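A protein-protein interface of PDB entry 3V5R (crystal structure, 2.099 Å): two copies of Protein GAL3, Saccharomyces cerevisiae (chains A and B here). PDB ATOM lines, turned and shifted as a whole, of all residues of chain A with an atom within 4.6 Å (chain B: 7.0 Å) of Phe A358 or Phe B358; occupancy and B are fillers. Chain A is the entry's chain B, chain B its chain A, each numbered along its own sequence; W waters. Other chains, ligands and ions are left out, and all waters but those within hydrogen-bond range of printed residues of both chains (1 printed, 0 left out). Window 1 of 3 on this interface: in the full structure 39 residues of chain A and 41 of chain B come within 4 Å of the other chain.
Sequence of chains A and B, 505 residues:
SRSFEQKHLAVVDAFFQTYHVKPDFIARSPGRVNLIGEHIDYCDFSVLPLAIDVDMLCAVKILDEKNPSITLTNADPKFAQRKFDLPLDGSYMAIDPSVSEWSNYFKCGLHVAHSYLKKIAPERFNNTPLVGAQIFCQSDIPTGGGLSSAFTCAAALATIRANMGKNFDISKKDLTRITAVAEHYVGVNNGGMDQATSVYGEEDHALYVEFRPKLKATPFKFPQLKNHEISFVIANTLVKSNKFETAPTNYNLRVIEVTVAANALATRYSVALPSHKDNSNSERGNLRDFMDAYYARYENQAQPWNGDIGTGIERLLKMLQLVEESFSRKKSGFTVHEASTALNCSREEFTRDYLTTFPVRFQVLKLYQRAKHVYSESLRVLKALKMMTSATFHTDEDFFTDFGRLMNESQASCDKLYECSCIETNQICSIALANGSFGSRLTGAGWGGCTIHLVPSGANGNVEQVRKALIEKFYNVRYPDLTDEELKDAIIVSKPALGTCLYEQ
The backbone carbonyl oxygen (O) of Val A360 sits close to the backbone NH (N) of Gly B187 (3.4 Å). The backbone carbonyl oxygen (O) of Leu A355 lies close to the side-chain amide oxygen (OD1) of Asn B189 (3.2 Å). The side-chain amide oxygen (OD1) of Asn B189 sits close to the backbone carbonyl oxygen (O) of Thr A356 (2.9 Å). ND2 of Asn B189 lies within hydrogen-bond range of O of Phe A358. The backbone carbonyl oxygen (O) of Thr A357 is in hydrogen-bond range of the side-chain hydroxyl (OH) of Tyr B251 (2.7 Å). The backbone carbonyl oxygen (O) of Thr B356 lies within hydrogen-bond range of the side-chain amide nitrogen (ND2) of Asn A189 (3.4 Å). The side-chain amide nitrogen of Asn A189 sits at hydrogen-bond distance from the backbone carbonyl oxygen of Thr B357, 2.6 Å away. O of Thr B357 lies within hydrogen-bond range of OH of Tyr A251.
ND2 of Asn B252 lies within hydrogen-bond range of O of Pro B359 (3.2 Å). The side-chain amide nitrogen of Asn A252 lies within hydrogen-bond range of the backbone carbonyl oxygen of Pro A359 (3.2 Å).
Among the printed residues, pairs that only touch across the chains: Asn A252 with Phe B358 (3.1 Å), Phe A358 with Asn B252 (3.2 Å), Phe A358 with Phe B358 (3.4 Å), Thr A357 with Val B255 (3.5 Å), Asn A189 with Pro B359 (3.5 Å), Pro A359 with Asn B189 (3.6 Å), Pro A359 with Gly B187 (3.6 Å) and Asn A189 with Phe B358 (3.8 Å).
Of the printed residues of chain A, Phe B358 touches Asn A189 (3.8 Å), Asn A252 (3.1 Å) and Phe A358 (3.4 Å). Of the printed residues of chain A, Thr B356 touches Asn A189. Printed residues of chain B within 4 Å of Thr A356: Asn B189 (2.9 Å). Printed residues of chain B within 4 Å of Asn A252: Phe B358 (3.1 Å). Arg B361 touches none of the printed residues of chain A. The nearest printed residue of chain A that does not touch Phe B358 is Tyr A251 (4.1 Å).
Of the 17 printed residues of chain B, 9 touch a printed residue of chain A. Hydrophobic or aromatic side chains of chain A that line the printed part of chain B: Tyr A251, Phe A358 and Pro A359. Among the printed residues, no Asp or Glu carboxylate lies within 4 Å of a Lys or Arg side-chain nitrogen of the other chain.
Asn A189 touches Thr B356, and with the chains exchanged Thr A356 touches Asn B189. Asn A189 touches Phe B358, and with the chains exchanged Phe A358 touches Asn B189. Asn A189 touches Pro B359, and with the chains exchanged Pro A359 touches Asn B189. Asn A252 touches Phe B358, and with the chains exchanged Phe A358 touches Asn B252. Positions printed for both chains: 189, 251, 252, 355, 356, 357, 358, 359 and 360. Of the 16 pairs that touch across the chains among the printed residues, 11 have their exchanged pair printed and touching as well.
Water W1 lies within hydrogen-bond range of the backbone carbonyl oxygen of Val B188 (2.8 Å) and the backbone NH of Val A360 (2.9 Å).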
ATOM      1  N   ASN A 189      24.575  -3.274  21.640  1.00  0.00           N
ATOM      2  CA  ASN A 189      24.924  -1.859  21.671  1.00  0.00           C
ATOM      3  C   ASN A 189      23.940  -1.006  22.474  1.00  0.00           C
ATOM      4  O   ASN A 189      23.203  -0.191  21.929  1.00  0.00           O
ATOM      5  CB  ASN A 189      25.146  -1.310  20.251  1.00  0.00           C
ATOM      6  CG  ASN A 189      23.893  -1.352  19.399  1.00  0.00           C
ATOM      7  OD1 ASN A 189      23.063  -2.258  19.524  1.00  0.00           O
ATOM      8  ND2 ASN A 189      23.745  -0.361  18.532  1.00  0.00           N
ATOM      9  N   TYR A 251      14.810  -0.850  12.874  1.00  0.00           N
ATOM     10  CA  TYR A 251      15.874  -0.111  13.562  1.00  0.00           C
ATOM     11  C   TYR A 251      16.683   0.810  12.652  1.00  0.00           C
ATOM     12  O   TYR A 251      16.913   1.966  12.986  1.00  0.00           O
ATOM     13  CB  TYR A 251      16.839  -1.062  14.263  1.00  0.00           C
ATOM     14  CG  TYR A 251      17.960  -0.334  14.968  1.00  0.00           C
ATOM     15  CD1 TYR A 251      17.734   0.293  16.185  1.00  0.00           C
ATOM     16  CD2 TYR A 251      19.236  -0.273  14.422  1.00  0.00           C
ATOM     17  CE1 TYR A 251      18.738   0.957  16.841  1.00  0.00           C
ATOM     18  CE2 TYR A 251      20.257   0.397  15.072  1.00  0.00           C
ATOM     19  CZ  TYR A 251      19.995   1.009  16.287  1.00  0.00           C
ATOM     20  OH  TYR A 251      20.986   1.684  16.954  1.00  0.00           O
ATOM     21  N   ASN A 252      17.124   0.277  11.520  1.00  0.00           N
ATOM     22  CA  ASN A 252      17.908   1.048  10.552  1.00  0.00           C
ATOM     23  C   ASN A 252      17.165   2.274  10.061  1.00  0.00           C
ATOM     24  O   ASN A 252      17.742   3.347   9.900  1.00  0.00           O
ATOM     25  CB  ASN A 252      18.279   0.181   9.349  1.00  0.00           C
ATOM     26  CG  ASN A 252      19.218  -0.951   9.716  1.00  0.00           C
ATOM     27  OD1 ASN A 252      19.760  -0.987  10.825  1.00  0.00           O
ATOM     28  ND2 ASN A 252      19.425  -1.880   8.780  1.00  0.00           N
ATOM     29  N   LEU A 355      21.852   7.581   3.296  1.00  0.00           N
ATOM     30  CA  LEU A 355      21.294   6.317   2.808  1.00  0.00           C
ATOM     31  C   LEU A 355      22.346   5.300   2.338  1.00  0.00           C
ATOM     32  O   LEU A 355      22.012   4.342   1.640  1.00  0.00           O
ATOM     33  CB  LEU A 355      20.342   6.603   1.636  1.00  0.00           C
ATOM     34  CG  LEU A 355      19.195   7.584   1.878  1.00  0.00           C
ATOM     35  CD1 LEU A 355      18.329   7.684   0.621  1.00  0.00           C
ATOM     36  CD2 LEU A 355      18.372   7.129   3.067  1.00  0.00           C
ATOM     37  N   THR A 356      23.609   5.492   2.704  1.00  0.00           N
ATOM     38  CA  THR A 356      24.668   4.752   2.002  1.00  0.00           C
ATOM     39  C   THR A 356      24.987   3.344   2.480  1.00  0.00           C
ATOM     40  O   THR A 356      24.863   2.384   1.722  1.00  0.00           O
ATOM     41  CB  THR A 356      25.993   5.515   1.981  1.00  0.00           C
ATOM     42  OG1 THR A 356      26.107   6.299   3.174  1.00  0.00           O
ATOM     43  CG2 THR A 356      26.066   6.395   0.743  1.00  0.00           C
ATOM     44  N   THR A 357      25.447   3.218   3.715  1.00  0.00           N
ATOM     45  CA  THR A 357      26.073   1.965   4.117  1.00  0.00           C
ATOM     46  C   THR A 357      25.082   0.914   4.662  1.00  0.00           C
ATOM     47  O   THR A 357      25.283  -0.294   4.494  1.00  0.00           O
ATOM     48  CB  THR A 357      27.268   2.222   5.070  1.00  0.00           C
ATOM     49  OG1 THR A 357      28.320   2.883   4.347  1.00  0.00           O
ATOM     50  CG2 THR A 357      27.799   0.928   5.615  1.00  0.00           C
ATOM     51  N   PHE A 358      23.990   1.375   5.262  1.00  0.00           N
ATOM     52  CA  PHE A 358      23.028   0.452   5.854  1.00  0.00           C
ATOM     53  C   PHE A 358      21.672   0.376   5.134  1.00  0.00           C
ATOM     54  O   PHE A 358      21.058   1.392   4.804  1.00  0.00           O
ATOM     55  CB  PHE A 358      22.891   0.732   7.352  1.00  0.00           C
ATOM     56  CG  PHE A 358      24.180   0.535   8.110  1.00  0.00           C
ATOM     57  CD1 PHE A 358      24.450  -0.668   8.750  1.00  0.00           C
ATOM     58  CD2 PHE A 358      25.138   1.538   8.152  1.00  0.00           C
ATOM     59  CE1 PHE A 358      25.640  -0.859   9.441  1.00  0.00           C
ATOM     60  CE2 PHE A 358      26.330   1.352   8.841  1.00  0.00           C
ATOM     61  CZ  PHE A 358      26.580   0.147   9.485  1.00  0.00           C
ATOM     62  N   PRO A 359      21.204  -0.852   4.888  1.00  0.00           N
ATOM     63  CA  PRO A 359      20.003  -1.113   4.093  1.00  0.00           C
ATOM     64  C   PRO A 359      18.754  -0.516   4.725  1.00  0.00           C
ATOM     65  O   PRO A 359      18.581  -0.606   5.936  1.00  0.00           O
ATOM     66  CB  PRO A 359      19.895  -2.644   4.119  1.00  0.00           C
ATOM     67  CG  PRO A 359      21.240  -3.133   4.571  1.00  0.00           C
ATOM     68  CD  PRO A 359      21.759  -2.082   5.472  1.00  0.00           C
ATOM     69  N   VAL A 360      17.901   0.099   3.912  1.00  0.00           N
ATOM     70  CA  VAL A 360      16.632   0.619   4.404  1.00  0.00           C
ATOM     71  C   VAL A 360      15.503   0.458   3.393  1.00  0.00           C
ATOM     72  O   VAL A 360      15.727   0.438   2.185  1.00  0.00           O
ATOM     73  CB  VAL A 360      16.736   2.102   4.835  1.00  0.00           C
ATOM     74  CG1 VAL A 360      17.177   2.200   6.279  1.00  0.00           C
ATOM     75  CG2 VAL A 360      17.668   2.879   3.906  1.00  0.00           C
ATOM     76  N   GLY B 187      15.471  -2.055  -0.087  1.00  0.00           N
ATOM     77  CA  GLY B 187      16.169  -2.412   1.139  1.00  0.00           C
ATOM     78  C   GLY B 187      17.485  -3.068   0.809  1.00  0.00           C
ATOM     79  O   GLY B 187      17.900  -4.054   1.420  1.00  0.00           O
ATOM     80  N   VAL B 188      18.142  -2.492  -0.183  1.00  0.00           N
ATOM     81  CA  VAL B 188      19.373  -3.031  -0.713  1.00  0.00           C
ATOM     82  C   VAL B 188      20.354  -1.869  -0.862  1.00  0.00           C
ATOM     83  O   VAL B 188      19.940  -0.724  -1.041  1.00  0.00           O
ATOM     84  CB  VAL B 188      19.075  -3.754  -2.049  1.00  0.00           C
ATOM     85  CG1 VAL B 188      20.283  -3.778  -2.973  1.00  0.00           C
ATOM     86  CG2 VAL B 188      18.561  -5.163  -1.759  1.00  0.00           C
ATOM     87  N   ASN B 189      21.646  -2.140  -0.747  1.00  0.00           N
ATOM     88  CA  ASN B 189      22.598  -1.048  -0.825  1.00  0.00           C
ATOM     89  C   ASN B 189      23.837  -1.325  -1.661  1.00  0.00           C
ATOM     90  O   ASN B 189      24.953  -1.382  -1.139  1.00  0.00           O
ATOM     91  CB  ASN B 189      22.967  -0.562   0.573  1.00  0.00           C
ATOM     92  CG  ASN B 189      22.531   0.862   0.805  1.00  0.00           C
ATOM     93  OD1 ASN B 189      22.699   1.718  -0.069  1.00  0.00           O
ATOM     94  ND2 ASN B 189      21.953   1.127   1.968  1.00  0.00           N
ATOM     95  N   PRO B 248      26.491  -9.215  13.604  1.00  0.00           N
ATOM     96  CA  PRO B 248      27.402  -8.244  14.216  1.00  0.00           C
ATOM     97  C   PRO B 248      28.855  -8.601  13.970  1.00  0.00           C
ATOM     98  O   PRO B 248      29.729  -7.766  14.182  1.00  0.00           O
ATOM     99  CB  PRO B 248      27.092  -8.375  15.719  1.00  0.00           C
ATOM    100  CG  PRO B 248      25.723  -8.949  15.778  1.00  0.00           C
ATOM    101  CD  PRO B 248      25.638  -9.877  14.607  1.00  0.00           C
ATOM    102  N   TYR B 251      28.926  -8.010   8.164  1.00  0.00           N
ATOM    103  CA  TYR B 251      28.940  -6.755   7.404  1.00  0.00           C
ATOM    104  C   TYR B 251      29.213  -5.504   8.241  1.00  0.00           C
ATOM    105  O   TYR B 251      30.060  -4.688   7.869  1.00  0.00           O
ATOM    106  CB  TYR B 251      27.646  -6.573   6.602  1.00  0.00           C
ATOM    107  CG  TYR B 251      27.603  -5.269   5.837  1.00  0.00           C
ATOM    108  CD1 TYR B 251      28.297  -5.121   4.647  1.00  0.00           C
ATOM    109  CD2 TYR B 251      26.874  -4.189   6.307  1.00  0.00           C
ATOM    110  CE1 TYR B 251      28.259  -3.939   3.942  1.00  0.00           C
ATOM    111  CE2 TYR B 251      26.843  -3.001   5.619  1.00  0.00           C
ATOM    112  CZ  TYR B 251      27.532  -2.886   4.433  1.00  0.00           C
ATOM    113  OH  TYR B 251      27.500  -1.704   3.739  1.00  0.00           O
ATOM    114  N   ASN B 252      28.493  -5.345   9.354  1.00  0.00           N
ATOM    115  CA  ASN B 252      28.715  -4.214  10.256  1.00  0.00           C
ATOM    116  C   ASN B 252      30.162  -4.151  10.712  1.00  0.00           C
ATOM    117  O   ASN B 252      30.740  -3.086  10.781  1.00  0.00           O
ATOM    118  CB  ASN B 252      27.838  -4.306  11.502  1.00  0.00           C
ATOM    119  CG  ASN B 252      26.360  -4.304  11.185  1.00  0.00           C
ATOM    120  OD1 ASN B 252      25.940  -3.945  10.082  1.00  0.00           O
ATOM    121  ND2 ASN B 252      25.555  -4.699  12.168  1.00  0.00           N
ATOM    122  N   LEU B 253      30.733  -5.302  11.045  1.00  0.00           N
ATOM    123  CA  LEU B 253      32.122  -5.346  11.467  1.00  0.00           C
ATOM    124  C   LEU B 253      33.062  -4.921  10.336  1.00  0.00           C
ATOM    125  O   LEU B 253      34.005  -4.174  10.568  1.00  0.00           O
ATOM    126  CB  LEU B 253      32.502  -6.734  12.013  1.00  0.00           C
ATOM    127  CG  LEU B 253      33.973  -6.886  12.457  1.00  0.00           C
ATOM    128  CD1 LEU B 253      34.406  -5.784  13.423  1.00  0.00           C
ATOM    129  CD2 LEU B 253      34.275  -8.282  13.045  1.00  0.00           C
ATOM    130  N   VAL B 255      32.436  -2.869   7.785  1.00  0.00           N
ATOM    131  CA  VAL B 255      32.283  -1.431   7.578  1.00  0.00           C
ATOM    132  C   VAL B 255      33.115  -0.637   8.585  1.00  0.00           C
ATOM    133  O   VAL B 255      33.720   0.392   8.259  1.00  0.00           O
ATOM    134  CB  VAL B 255      30.814  -1.005   7.711  1.00  0.00           C
ATOM    135  CG1 VAL B 255      30.687   0.515   7.642  1.00  0.00           C
ATOM    136  CG2 VAL B 255      29.982  -1.658   6.621  1.00  0.00           C
ATOM    137  N   ILE B 256      33.133  -1.121   9.826  1.00  0.00           N
ATOM    138  CA  ILE B 256      33.917  -0.456  10.859  1.00  0.00           C
ATOM    139  C   ILE B 256      35.384  -0.626  10.552  1.00  0.00           C
ATOM    140  O   ILE B 256      36.151   0.328  10.600  1.00  0.00           O
ATOM    141  CB  ILE B 256      33.683  -1.057  12.263  1.00  0.00           C
ATOM    142  CG1 ILE B 256      32.241  -0.866  12.708  1.00  0.00           C
ATOM    143  CG2 ILE B 256      34.603  -0.406  13.269  1.00  0.00           C
ATOM    144  CD1 ILE B 256      31.743   0.498  12.489  1.00  0.00           C
ATOM    145  N   TYR B 354      32.840   4.906  16.368  1.00  0.00           N
ATOM    146  CA  TYR B 354      32.772   3.642  15.624  1.00  0.00           C
ATOM    147  C   TYR B 354      31.919   2.550  16.227  1.00  0.00           C
ATOM    148  O   TYR B 354      31.553   1.608  15.540  1.00  0.00           O
ATOM    149  CB  TYR B 354      34.172   3.084  15.407  1.00  0.00           C
ATOM    150  CG  TYR B 354      35.021   3.986  14.580  1.00  0.00           C
ATOM    151  CD1 TYR B 354      34.884   4.002  13.204  1.00  0.00           C
ATOM    152  CD2 TYR B 354      35.952   4.837  15.163  1.00  0.00           C
ATOM    153  CE1 TYR B 354      35.642   4.822  12.427  1.00  0.00           C
ATOM    154  CE2 TYR B 354      36.728   5.671  14.387  1.00  0.00           C
ATOM    155  CZ  TYR B 354      36.558   5.650  13.007  1.00  0.00           C
ATOM    156  OH  TYR B 354      37.298   6.458  12.187  1.00  0.00           O
ATOM    157  N   LEU B 355      31.617   2.645  17.511  1.00  0.00           N
ATOM    158  CA  LEU B 355      30.956   1.524  18.157  1.00  0.00           C
ATOM    159  C   LEU B 355      29.569   1.895  18.654  1.00  0.00           C
ATOM    160  O   LEU B 355      29.010   1.212  19.502  1.00  0.00           O
ATOM    161  CB  LEU B 355      31.819   0.999  19.311  1.00  0.00           C
ATOM    162  CG  LEU B 355      33.241   0.559  18.935  1.00  0.00           C
ATOM    163  CD1 LEU B 355      34.067   0.229  20.174  1.00  0.00           C
ATOM    164  CD2 LEU B 355      33.182  -0.637  18.010  1.00  0.00           C
ATOM    165  N   THR B 356      29.005   2.971  18.123  1.00  0.00           N
ATOM    166  CA  THR B 356      27.786   3.510  18.718  1.00  0.00           C
ATOM    167  C   THR B 356      26.486   3.033  18.082  1.00  0.00           C
ATOM    168  O   THR B 356      25.598   2.532  18.767  1.00  0.00           O
ATOM    169  CB  THR B 356      27.792   5.041  18.705  1.00  0.00           C
ATOM    170  OG1 THR B 356      28.388   5.496  17.483  1.00  0.00           O
ATOM    171  CG2 THR B 356      28.581   5.576  19.896  1.00  0.00           C
ATOM    172  N   THR B 357      26.364   3.204  16.777  1.00  0.00           N
ATOM    173  CA  THR B 357      25.066   3.019  16.153  1.00  0.00           C
ATOM    174  C   THR B 357      24.684   1.553  15.962  1.00  0.00           C
ATOM    175  O   THR B 357      23.640   1.114  16.442  1.00  0.00           O
ATOM    176  CB  THR B 357      24.973   3.764  14.817  1.00  0.00           C
ATOM    177  OG1 THR B 357      25.465   5.102  14.983  1.00  0.00           O
ATOM    178  CG2 THR B 357      23.531   3.806  14.352  1.00  0.00           C
ATOM    179  N   PHE B 358      25.537   0.798  15.281  1.00  0.00           N
ATOM    180  CA  PHE B 358      25.201  -0.574  14.915  1.00  0.00           C
ATOM    181  C   PHE B 358      25.950  -1.631  15.737  1.00  0.00           C
ATOM    182  O   PHE B 358      27.100  -1.428  16.125  1.00  0.00           O
ATOM    183  CB  PHE B 358      25.385  -0.761  13.407  1.00  0.00           C
ATOM    184  CG  PHE B 358      24.474   0.123  12.579  1.00  0.00           C
ATOM    185  CD1 PHE B 358      23.185  -0.288  12.256  1.00  0.00           C
ATOM    186  CD2 PHE B 358      24.894   1.373  12.148  1.00  0.00           C
ATOM    187  CE1 PHE B 358      22.341   0.527  11.504  1.00  0.00           C
ATOM    188  CE2 PHE B 358      24.052   2.191  11.395  1.00  0.00           C
ATOM    189  CZ  PHE B 358      22.775   1.765  11.077  1.00  0.00           C
ATOM    190  N   PRO B 359      25.279  -2.756  16.030  1.00  0.00           N
ATOM    191  CA  PRO B 359      25.852  -3.812  16.869  1.00  0.00           C
ATOM    192  C   PRO B 359      27.039  -4.465  16.185  1.00  0.00           C
ATOM    193  O   PRO B 359      26.971  -4.747  14.994  1.00  0.00           O
ATOM    194  CB  PRO B 359      24.709  -4.832  16.982  1.00  0.00           C
ATOM    195  CG  PRO B 359      23.479  -4.108  16.536  1.00  0.00           C
ATOM    196  CD  PRO B 359      23.938  -3.113  15.541  1.00  0.00           C
ATOM    197  N   VAL B 360      28.118  -4.692  16.927  1.00  0.00           N
ATOM    198  CA  VAL B 360      29.280  -5.383  16.377  1.00  0.00           C
ATOM    199  C   VAL B 360      29.885  -6.313  17.405  1.00  0.00           C
ATOM    200  O   VAL B 360      29.774  -6.087  18.610  1.00  0.00           O
ATOM    201  CB  VAL B 360      30.383  -4.414  15.888  1.00  0.00           C
ATOM    202  CG1 VAL B 360      30.035  -3.846  14.532  1.00  0.00           C
ATOM    203  CG2 VAL B 360      30.639  -3.301  16.919  1.00  0.00           C
ATOM    204  N   ARG B 361      30.532  -7.363  16.926  1.00  0.00           N
ATOM    205  CA  ARG B 361      31.130  -8.330  17.828  1.00  0.00           C
ATOM    206  C   ARG B 361      32.515  -8.711  17.349  1.00  0.00           C
ATOM    207  O   ARG B 361      32.682  -9.243  16.252  1.00  0.00           O
ATOM    208  CB  ARG B 361      30.249  -9.572  17.929  1.00  0.00           C
ATOM    209  CG  ARG B 361      30.816 -10.661  18.841  1.00  0.00           C
ATOM    210  CD  ARG B 361      29.897 -11.871  18.899  1.00  0.00           C
ATOM    211  NE  ARG B 361      28.512 -11.470  19.123  1.00  0.00           N
ATOM    212  CZ  ARG B 361      27.506 -11.757  18.303  1.00  0.00           C
ATOM    213  NH1 ARG B 361      27.725 -12.466  17.201  1.00  0.00           N
ATOM    214  NH2 ARG B 361      26.276 -11.344  18.591  1.00  0.00           N
HETATM  215  O   HOH W   1      18.491   0.433   1.095  1.00  0.00           O
